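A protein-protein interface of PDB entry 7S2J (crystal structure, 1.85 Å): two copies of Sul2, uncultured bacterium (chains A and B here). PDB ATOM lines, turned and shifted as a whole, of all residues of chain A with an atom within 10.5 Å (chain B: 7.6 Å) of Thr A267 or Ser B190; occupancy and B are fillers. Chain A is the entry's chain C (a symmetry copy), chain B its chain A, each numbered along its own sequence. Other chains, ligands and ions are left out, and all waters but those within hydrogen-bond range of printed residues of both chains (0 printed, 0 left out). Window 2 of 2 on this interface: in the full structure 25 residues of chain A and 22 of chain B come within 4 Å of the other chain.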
ATOM      1  N   ALA A 259      16.472 -14.205 -15.258  1.00  0.00           N
ATOM      2  CA  ALA A 259      15.207 -14.672 -14.700  1.00  0.00           C
ATOM      3  C   ALA A 259      14.406 -15.445 -15.736  1.00  0.00           C
ATOM      4  O   ALA A 259      13.741 -16.428 -15.395  1.00  0.00           O
ATOM      5  CB  ALA A 259      14.390 -13.500 -14.158  1.00  0.00           C
ATOM      6  N   VAL A 260      14.498 -15.039 -17.004  1.00  0.00           N
ATOM      7  CA  VAL A 260      13.853 -15.786 -18.081  1.00  0.00           C
ATOM      8  C   VAL A 260      14.500 -17.154 -18.233  1.00  0.00           C
ATOM      9  O   VAL A 260      13.812 -18.179 -18.306  1.00  0.00           O
ATOM     10  CB  VAL A 260      13.915 -14.995 -19.401  1.00  0.00           C
ATOM     11  CG1 VAL A 260      13.569 -15.909 -20.584  1.00  0.00           C
ATOM     12  CG2 VAL A 260      13.006 -13.788 -19.346  1.00  0.00           C
ATOM     13  N   LEU A 261      15.833 -17.197 -18.277  1.00  0.00           N
ATOM     14  CA  LEU A 261      16.513 -18.479 -18.430  1.00  0.00           C
ATOM     15  C   LEU A 261      16.264 -19.395 -17.233  1.00  0.00           C
ATOM     16  O   LEU A 261      16.157 -20.618 -17.398  1.00  0.00           O
ATOM     17  CB  LEU A 261      18.018 -18.271 -18.640  1.00  0.00           C
ATOM     18  CG  LEU A 261      18.466 -17.470 -19.869  1.00  0.00           C
ATOM     19  CD1 LEU A 261      19.951 -17.693 -20.113  1.00  0.00           C
ATOM     20  CD2 LEU A 261      17.641 -17.796 -21.116  1.00  0.00           C
ATOM     21  N   ALA A 262      16.156 -18.829 -16.022  1.00  0.00           N
ATOM     22  CA  ALA A 262      15.885 -19.664 -14.848  1.00  0.00           C
ATOM     23  C   ALA A 262      14.479 -20.252 -14.890  1.00  0.00           C
ATOM     24  O   ALA A 262      14.281 -21.426 -14.541  1.00  0.00           O
ATOM     25  CB  ALA A 262      16.080 -18.866 -13.552  1.00  0.00           C
ATOM     26  N   ALA A 263      13.487 -19.452 -15.287  1.00  0.00           N
ATOM     27  CA  ALA A 263      12.126 -19.971 -15.367  1.00  0.00           C
ATOM     28  C   ALA A 263      12.016 -21.039 -16.443  1.00  0.00           C
ATOM     29  O   ALA A 263      11.291 -22.026 -16.274  1.00  0.00           O
ATOM     30  CB  ALA A 263      11.134 -18.837 -15.625  1.00  0.00           C
ATOM     31  N   LEU A 264      12.736 -20.863 -17.552  1.00  0.00           N
ATOM     32  CA  LEU A 264      12.739 -21.877 -18.600  1.00  0.00           C
ATOM     33  C   LEU A 264      13.383 -23.170 -18.114  1.00  0.00           C
ATOM     34  O   LEU A 264      12.875 -24.264 -18.384  1.00  0.00           O
ATOM     35  CB  LEU A 264      13.472 -21.348 -19.833  1.00  0.00           C
ATOM     36  CG  LEU A 264      12.695 -20.335 -20.674  1.00  0.00           C
ATOM     37  CD1 LEU A 264      13.572 -19.775 -21.778  1.00  0.00           C
ATOM     38  CD2 LEU A 264      11.429 -20.987 -21.246  1.00  0.00           C
ATOM     39  N   LYS A 265      14.514 -23.063 -17.414  1.00  0.00           N
ATOM     40  CA  LYS A 265      15.189 -24.254 -16.899  1.00  0.00           C
ATOM     41  C   LYS A 265      14.311 -24.977 -15.887  1.00  0.00           C
ATOM     42  O   LYS A 265      14.206 -26.212 -15.904  1.00  0.00           O
ATOM     43  CB  LYS A 265      16.532 -23.862 -16.270  1.00  0.00           C
ATOM     44  CG  LYS A 265      17.441 -25.039 -15.918  1.00  0.00           C
ATOM     45  CD  LYS A 265      18.906 -24.617 -15.804  1.00  0.00           C
ATOM     46  CE  LYS A 265      19.376 -24.647 -14.349  1.00  0.00           C
ATOM     47  NZ  LYS A 265      20.864 -24.644 -14.212  1.00  0.00           N
ATOM     48  N   GLU A 266      13.660 -24.217 -15.002  1.00  0.00           N
ATOM     49  CA  GLU A 266      12.748 -24.818 -14.038  1.00  0.00           C
ATOM     50  C   GLU A 266      11.573 -25.490 -14.732  1.00  0.00           C
ATOM     51  O   GLU A 266      11.124 -26.564 -14.309  1.00  0.00           O
ATOM     52  CB  GLU A 266      12.257 -23.762 -13.051  1.00  0.00           C
ATOM     53  CG  GLU A 266      11.305 -24.284 -11.962  1.00  0.00           C
ATOM     54  CD  GLU A 266      11.810 -25.491 -11.157  1.00  0.00           C
ATOM     55  OE1 GLU A 266      12.964 -25.941 -11.329  1.00  0.00           O
ATOM     56  OE2 GLU A 266      11.014 -26.015 -10.351  1.00  0.00           O
ATOM     57  N   THR A 267      11.058 -24.870 -15.798  1.00  0.00           N
ATOM     58  CA  THR A 267       9.972 -25.477 -16.567  1.00  0.00           C
ATOM     59  C   THR A 267      10.399 -26.818 -17.151  1.00  0.00           C
ATOM     60  O   THR A 267       9.634 -27.791 -17.125  1.00  0.00           O
ATOM     61  CB  THR A 267       9.536 -24.538 -17.692  1.00  0.00           C
ATOM     62  OG1 THR A 267       9.081 -23.294 -17.146  1.00  0.00           O
ATOM     63  CG2 THR A 267       8.414 -25.173 -18.483  1.00  0.00           C
ATOM     64  N   ALA A 268      11.625 -26.885 -17.677  1.00  0.00           N
ATOM     65  CA  ALA A 268      12.089 -28.098 -18.341  1.00  0.00           C
ATOM     66  C   ALA A 268      12.414 -29.189 -17.332  1.00  0.00           C
ATOM     67  O   ALA A 268      12.182 -30.375 -17.595  1.00  0.00           O
ATOM     68  CB  ALA A 268      13.303 -27.784 -19.215  1.00  0.00           C
ATOM     69  N   ARG A 269      12.945 -28.811 -16.167  1.00  0.00           N
ATOM     70  CA  ARG A 269      13.273 -29.808 -15.154  1.00  0.00           C
ATOM     71  C   ARG A 269      12.016 -30.448 -14.575  1.00  0.00           C
ATOM     72  O   ARG A 269      11.961 -31.672 -14.400  1.00  0.00           O
ATOM     73  CB  ARG A 269      14.120 -29.176 -14.049  1.00  0.00           C
ATOM     74  CG  ARG A 269      14.056 -29.908 -12.715  1.00  0.00           C
ATOM     75  CD  ARG A 269      14.224 -28.953 -11.542  1.00  0.00           C
ATOM     76  NE  ARG A 269      13.969 -29.608 -10.266  1.00  0.00           N
ATOM     77  CZ  ARG A 269      12.807 -29.577  -9.628  1.00  0.00           C
ATOM     78  NH1 ARG A 269      11.777 -28.893 -10.103  1.00  0.00           N
ATOM     79  NH2 ARG A 269      12.674 -30.245  -8.485  1.00  0.00           N
ATOM     80  N   ILE A 270      10.996 -29.645 -14.280  1.00  0.00           N
ATOM     81  CA  ILE A 270       9.761 -30.166 -13.706  1.00  0.00           C
ATOM     82  C   ILE A 270       8.936 -30.854 -14.787  1.00  0.00           C
ATOM     83  O   ILE A 270       9.108 -32.045 -15.051  1.00  0.00           O
ATOM     84  CB  ILE A 270       8.940 -29.055 -13.022  1.00  0.00           C
ATOM     85  CG1 ILE A 270       7.773 -29.659 -12.241  1.00  0.00           C
ATOM     86  CG2 ILE A 270       8.397 -28.083 -14.055  1.00  0.00           C
ATOM     87  CD1 ILE A 270       7.351 -28.841 -11.037  1.00  0.00           C
ATOM     88  N   ASP B 145      -1.876 -31.357 -20.101  1.00  0.00           N
ATOM     89  CA  ASP B 145      -0.633 -30.788 -20.603  1.00  0.00           C
ATOM     90  C   ASP B 145      -0.905 -29.920 -21.829  1.00  0.00           C
ATOM     91  O   ASP B 145      -1.419 -30.409 -22.836  1.00  0.00           O
ATOM     92  CB  ASP B 145       0.324 -31.934 -20.937  1.00  0.00           C
ATOM     93  CG  ASP B 145       1.712 -31.468 -21.389  1.00  0.00           C
ATOM     94  OD1 ASP B 145       1.936 -30.273 -21.671  1.00  0.00           O
ATOM     95  OD2 ASP B 145       2.597 -32.342 -21.487  1.00  0.00           O
ATOM     96  N   ILE B 146      -0.513 -28.638 -21.761  1.00  0.00           N
ATOM     97  CA  ILE B 146      -0.778 -27.716 -22.868  1.00  0.00           C
ATOM     98  C   ILE B 146      -0.173 -28.229 -24.169  1.00  0.00           C
ATOM     99  O   ILE B 146      -0.768 -28.078 -25.245  1.00  0.00           O
ATOM    100  CB  ILE B 146      -0.254 -26.304 -22.527  1.00  0.00           C
ATOM    101  CG1 ILE B 146      -0.556 -25.333 -23.673  1.00  0.00           C
ATOM    102  CG2 ILE B 146       1.246 -26.321 -22.231  1.00  0.00           C
ATOM    103  CD1 ILE B 146      -2.025 -24.971 -23.791  1.00  0.00           C
ATOM    104  N   MET B 147       1.031 -28.815 -24.101  1.00  0.00           N
ATOM    105  CA  MET B 147       1.655 -29.367 -25.305  1.00  0.00           C
ATOM    106  C   MET B 147       0.814 -30.475 -25.932  1.00  0.00           C
ATOM    107  O   MET B 147       0.770 -30.597 -27.161  1.00  0.00           O
ATOM    108  CB  MET B 147       3.063 -29.875 -24.987  1.00  0.00           C
ATOM    109  CG  MET B 147       4.153 -28.826 -24.782  1.00  0.00           C
ATOM    110  SD  MET B 147       3.995 -27.317 -25.747  1.00  0.00           S
ATOM    111  CE  MET B 147       4.394 -27.949 -27.381  1.00  0.00           C
ATOM    112  N   ILE B 150      -1.983 -28.652 -27.838  1.00  0.00           N
ATOM    113  CA  ILE B 150      -1.469 -28.025 -29.049  1.00  0.00           C
ATOM    114  C   ILE B 150      -1.136 -29.065 -30.120  1.00  0.00           C
ATOM    115  O   ILE B 150      -1.422 -28.860 -31.316  1.00  0.00           O
ATOM    116  CB  ILE B 150      -0.248 -27.148 -28.706  1.00  0.00           C
ATOM    117  CG1 ILE B 150      -0.670 -26.037 -27.736  1.00  0.00           C
ATOM    118  CG2 ILE B 150       0.332 -26.546 -29.977  1.00  0.00           C
ATOM    119  CD1 ILE B 150       0.461 -25.082 -27.348  1.00  0.00           C
ATOM    120  N   MET B 177       1.077 -17.784 -27.910  1.00  0.00           N
ATOM    121  CA  MET B 177       1.845 -17.339 -26.754  1.00  0.00           C
ATOM    122  C   MET B 177       1.029 -16.348 -25.941  1.00  0.00           C
ATOM    123  O   MET B 177       0.157 -15.659 -26.474  1.00  0.00           O
ATOM    124  CB  MET B 177       3.185 -16.722 -27.174  1.00  0.00           C
ATOM    125  CG  MET B 177       4.025 -16.386 -25.991  1.00  0.00           C
ATOM    126  SD  MET B 177       4.878 -17.852 -25.380  1.00  0.00           S
ATOM    127  CE  MET B 177       5.051 -18.917 -26.794  1.00  0.00           C
ATOM    128  N   LEU B 181      -2.619 -18.651 -24.928  1.00  0.00           N
ATOM    129  CA  LEU B 181      -2.391 -19.923 -24.243  1.00  0.00           C
ATOM    130  C   LEU B 181      -3.043 -20.013 -22.882  1.00  0.00           C
ATOM    131  O   LEU B 181      -3.360 -21.115 -22.437  1.00  0.00           O
ATOM    132  CB  LEU B 181      -0.894 -20.177 -24.043  1.00  0.00           C
ATOM    133  CG  LEU B 181      -0.048 -20.244 -25.292  1.00  0.00           C
ATOM    134  CD1 LEU B 181       1.404 -20.377 -24.825  1.00  0.00           C
ATOM    135  CD2 LEU B 181      -0.491 -21.408 -26.183  1.00  0.00           C
ATOM    136  N   ALA B 184      -1.852 -17.880 -17.079  1.00  0.00           N
ATOM    137  CA  ALA B 184      -0.718 -18.082 -16.183  1.00  0.00           C
ATOM    138  C   ALA B 184       0.604 -18.007 -16.954  1.00  0.00           C
ATOM    139  O   ALA B 184       0.701 -18.512 -18.076  1.00  0.00           O
ATOM    140  CB  ALA B 184      -0.830 -19.432 -15.475  1.00  0.00           C
ATOM    141  N   PRO B 185       1.644 -17.383 -16.394  1.00  0.00           N
ATOM    142  CA  PRO B 185       2.923 -17.335 -17.122  1.00  0.00           C
ATOM    143  C   PRO B 185       3.524 -18.710 -17.344  1.00  0.00           C
ATOM    144  O   PRO B 185       4.190 -18.921 -18.362  1.00  0.00           O
ATOM    145  CB  PRO B 185       3.808 -16.452 -16.226  1.00  0.00           C
ATOM    146  CG  PRO B 185       2.814 -15.634 -15.413  1.00  0.00           C
ATOM    147  CD  PRO B 185       1.684 -16.598 -15.150  1.00  0.00           C
ATOM    148  N   GLU B 186       3.288 -19.656 -16.425  1.00  0.00           N
ATOM    149  CA  GLU B 186       3.820 -21.009 -16.576  1.00  0.00           C
ATOM    150  C   GLU B 186       3.399 -21.646 -17.896  1.00  0.00           C
ATOM    151  O   GLU B 186       4.168 -22.413 -18.489  1.00  0.00           O
ATOM    152  CB  GLU B 186       3.359 -21.891 -15.412  1.00  0.00           C
ATOM    153  CG  GLU B 186       3.713 -21.344 -14.031  1.00  0.00           C
ATOM    154  CD  GLU B 186       2.604 -20.478 -13.453  1.00  0.00           C
ATOM    155  OE1 GLU B 186       1.701 -21.027 -12.778  1.00  0.00           O
ATOM    156  OE2 GLU B 186       2.625 -19.250 -13.688  1.00  0.00           O
ATOM    157  N   THR B 187       2.181 -21.359 -18.368  1.00  0.00           N
ATOM    158  CA  THR B 187       1.724 -21.952 -19.621  1.00  0.00           C
ATOM    159  C   THR B 187       2.569 -21.476 -20.796  1.00  0.00           C
ATOM    160  O   THR B 187       2.993 -22.278 -21.633  1.00  0.00           O
ATOM    161  CB  THR B 187       0.243 -21.623 -19.846  1.00  0.00           C
ATOM    162  OG1 THR B 187      -0.488 -21.812 -18.616  1.00  0.00           O
ATOM    163  CG2 THR B 187      -0.355 -22.498 -20.937  1.00  0.00           C
ATOM    164  N   SER B 188       2.827 -20.168 -20.875  1.00  0.00           N
ATOM    165  CA  SER B 188       3.661 -19.647 -21.952  1.00  0.00           C
ATOM    166  C   SER B 188       5.101 -20.145 -21.829  1.00  0.00           C
ATOM    167  O   SER B 188       5.753 -20.432 -22.841  1.00  0.00           O
ATOM    168  CB  SER B 188       3.621 -18.118 -21.944  1.00  0.00           C
ATOM    169  OG  SER B 188       2.359 -17.661 -22.396  1.00  0.00           O
ATOM    170  N   LEU B 189       5.610 -20.250 -20.595  1.00  0.00           N
ATOM    171  CA  LEU B 189       6.956 -20.773 -20.386  1.00  0.00           C
ATOM    172  C   LEU B 189       7.066 -22.229 -20.827  1.00  0.00           C
ATOM    173  O   LEU B 189       8.097 -22.637 -21.373  1.00  0.00           O
ATOM    174  CB  LEU B 189       7.352 -20.635 -18.916  1.00  0.00           C
ATOM    175  CG  LEU B 189       7.735 -19.222 -18.460  1.00  0.00           C
ATOM    176  CD1 LEU B 189       7.774 -19.180 -16.923  1.00  0.00           C
ATOM    177  CD2 LEU B 189       9.058 -18.773 -19.073  1.00  0.00           C
ATOM    178  N   SER B 190       6.019 -23.034 -20.592  1.00  0.00           N
ATOM    179  CA  SER B 190       6.044 -24.417 -21.072  1.00  0.00           C
ATOM    180  C   SER B 190       6.204 -24.468 -22.587  1.00  0.00           C
ATOM    181  O   SER B 190       7.026 -25.229 -23.112  1.00  0.00           O
ATOM    182  CB  SER B 190       4.773 -25.169 -20.651  1.00  0.00           C
ATOM    183  OG  SER B 190       4.661 -25.246 -19.246  1.00  0.00           O
ATOM    184  N   VAL B 191       5.416 -23.669 -23.303  1.00  0.00           N
ATOM    185  CA  VAL B 191       5.469 -23.669 -24.761  1.00  0.00           C
ATOM    186  C   VAL B 191       6.810 -23.131 -25.250  1.00  0.00           C
ATOM    187  O   VAL B 191       7.427 -23.697 -26.162  1.00  0.00           O
ATOM    188  CB  VAL B 191       4.277 -22.873 -25.320  1.00  0.00           C
ATOM    189  CG1 VAL B 191       4.426 -22.639 -26.825  1.00  0.00           C
ATOM    190  CG2 VAL B 191       2.959 -23.618 -25.001  1.00  0.00           C
ATOM    191  N   LEU B 192       7.292 -22.043 -24.649  1.00  0.00           N
ATOM    192  CA  LEU B 192       8.607 -21.520 -25.017  1.00  0.00           C
ATOM    193  C   LEU B 192       9.707 -22.551 -24.776  1.00  0.00           C
ATOM    194  O   LEU B 192      10.672 -22.629 -25.548  1.00  0.00           O
ATOM    195  CB  LEU B 192       8.891 -20.233 -24.237  1.00  0.00           C
ATOM    196  CG  LEU B 192      10.176 -19.453 -24.532  1.00  0.00           C
ATOM    197  CD1 LEU B 192      10.298 -19.086 -26.012  1.00  0.00           C
ATOM    198  CD2 LEU B 192      10.221 -18.198 -23.660  1.00  0.00           C
ATOM    199  N   ALA B 193       9.580 -23.354 -23.716  1.00  0.00           N
ATOM    200  CA  ALA B 193      10.570 -24.390 -23.436  1.00  0.00           C
ATOM    201  C   ALA B 193      10.417 -25.623 -24.325  1.00  0.00           C
ATOM    202  O   ALA B 193      11.411 -26.311 -24.595  1.00  0.00           O
ATOM    203  CB  ALA B 193      10.493 -24.823 -21.967  1.00  0.00           C
ATOM    204  N   ARG B 194       9.206 -25.944 -24.776  1.00  0.00           N
ATOM    205  CA  ARG B 194       8.969 -27.248 -25.390  1.00  0.00           C
ATOM    206  C   ARG B 194       8.474 -27.187 -26.833  1.00  0.00           C
ATOM    207  O   ARG B 194       8.097 -28.233 -27.380  1.00  0.00           O
ATOM    208  CB  ARG B 194       7.985 -28.074 -24.545  1.00  0.00           C
ATOM    209  CG  ARG B 194       8.388 -28.252 -23.069  1.00  0.00           C
ATOM    210  CD  ARG B 194       7.249 -28.844 -22.250  1.00  0.00           C
ATOM    211  NE  ARG B 194       6.776 -30.116 -22.790  1.00  0.00           N
ATOM    212  CZ  ARG B 194       5.634 -30.694 -22.444  1.00  0.00           C
ATOM    213  NH1 ARG B 194       4.839 -30.157 -21.531  1.00  0.00           N
ATOM    214  NH2 ARG B 194       5.269 -31.825 -23.044  1.00  0.00           N
ATOM    215  N   PHE B 195       8.472 -26.018 -27.479  1.00  0.00           N
ATOM    216  CA  PHE B 195       7.940 -25.965 -28.844  1.00  0.00           C
ATOM    217  C   PHE B 195       8.709 -26.860 -29.813  1.00  0.00           C
ATOM    218  O   PHE B 195       8.172 -27.223 -30.862  1.00  0.00           O
ATOM    219  CB  PHE B 195       7.952 -24.536 -29.386  1.00  0.00           C
ATOM    220  CG  PHE B 195       9.334 -24.021 -29.604  1.00  0.00           C
ATOM    221  CD1 PHE B 195       9.995 -24.238 -30.812  1.00  0.00           C
ATOM    222  CD2 PHE B 195       9.990 -23.355 -28.589  1.00  0.00           C
ATOM    223  CE1 PHE B 195      11.293 -23.793 -30.984  1.00  0.00           C
ATOM    224  CE2 PHE B 195      11.285 -22.915 -28.752  1.00  0.00           C
ATOM    225  CZ  PHE B 195      11.929 -23.122 -29.952  1.00  0.00           C
ATOM    226  N   ASP B 196       9.955 -27.223 -29.518  1.00  0.00           N
ATOM    227  CA  ASP B 196      10.626 -28.096 -30.474  1.00  0.00           C
ATOM    228  C   ASP B 196      10.000 -29.486 -30.524  1.00  0.00           C
ATOM    229  O   ASP B 196      10.208 -30.201 -31.507  1.00  0.00           O
ATOM    230  CB  ASP B 196      12.127 -28.156 -30.187  1.00  0.00           C
ATOM    231  CG  ASP B 196      12.886 -28.964 -31.228  1.00  0.00           C
ATOM    232  OD1 ASP B 196      13.028 -28.486 -32.379  1.00  0.00           O
ATOM    233  OD2 ASP B 196      13.405 -30.044 -30.867  1.00  0.00           O
ATOM    234  N   GLU B 197       9.212 -29.867 -29.515  1.00  0.00           N
ATOM    235  CA  GLU B 197       8.465 -31.121 -29.611  1.00  0.00           C
ATOM    236  C   GLU B 197       7.527 -31.119 -30.820  1.00  0.00           C
ATOM    237  O   GLU B 197       7.264 -32.179 -31.404  1.00  0.00           O
ATOM    238  CB  GLU B 197       7.675 -31.366 -28.315  1.00  0.00           C
ATOM    239  CG  GLU B 197       8.536 -31.358 -27.059  1.00  0.00           C
ATOM    240  CD  GLU B 197       7.735 -31.569 -25.778  1.00  0.00           C
ATOM    241  OE1 GLU B 197       6.521 -31.835 -25.871  1.00  0.00           O
ATOM    242  OE2 GLU B 197       8.333 -31.501 -24.677  1.00  0.00           O
ATOM    243  N   PHE B 215       3.440 -12.087 -19.932  1.00  0.00           N
ATOM    244  CA  PHE B 215       4.068 -13.036 -19.018  1.00  0.00           C
ATOM    245  C   PHE B 215       5.533 -12.692 -18.761  1.00  0.00           C
ATOM    246  O   PHE B 215       6.061 -13.019 -17.694  1.00  0.00           O
ATOM    247  CB  PHE B 215       3.934 -14.466 -19.542  1.00  0.00           C
ATOM    248  CG  PHE B 215       4.879 -14.808 -20.664  1.00  0.00           C
ATOM    249  CD1 PHE B 215       4.603 -14.425 -21.965  1.00  0.00           C
ATOM    250  CD2 PHE B 215       6.032 -15.533 -20.418  1.00  0.00           C
ATOM    251  CE1 PHE B 215       5.467 -14.750 -22.996  1.00  0.00           C
ATOM    252  CE2 PHE B 215       6.893 -15.858 -21.441  1.00  0.00           C
ATOM    253  CZ  PHE B 215       6.614 -15.469 -22.730  1.00  0.00           C
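The backbone carbonyl oxygen of Ala A263 lies within hydrogen-bond range of the side-chain hydroxyl of Thr A267, 2.7 Å away. O of Glu B186 is in hydrogen-bond range of OG of Ser B190, 3.0 Å away.
CB of Ala A263 touches CD1 of Leu B189 (3.6 Å). Leu A264 touches Leu B189 (CD2 to O, 3.7 Å). CG of Leu B192 touches CD2 of Leu A264, 3.8 Å away. CD2 of Leu A264 touches N of Ala B193, at 3.9 Å. Thr A267 touches Leu B189 (OG1 to CB, 3.6 Å). Thr A267 touches Ser B190 (CG2 to CA, 3.6 Å).
Of chain B, only Leu B189 and Ser B190 come within 4 Å of Thr A267. Of chain A, only Thr A267 (3.6 Å) comes within 4 Å of Ser B190. No residue of chain A comes within 4 Å of Thr B187. Of the printed residues of chain A, Leu B189 touches Ala A263, Leu A264 and Thr A267. No residue of chain A comes within 4 Å of Val B191. Printed residues of chain B within 4 Å of Leu A264: Leu B189, Leu B192 and Ala B193. Of the printed residues of chain B, Ala A263 touches Leu B189. Of the printed residues of chain A, Leu B192 touches Leu A264. Ala A268 touches none of the printed residues of chain B. Ile A270 touches none of the printed residues of chain B. The nearest residue of chain B that does not touch Thr A267 is Ala B193 (4.1 Å).
Hydrophobic or aromatic side chains of chain A that line the printed part of chain B: Ala A263 and Leu A264. Of the 21 printed residues of chain B, 4 touch a printed residue of chain A.
No position is printed for both chains.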
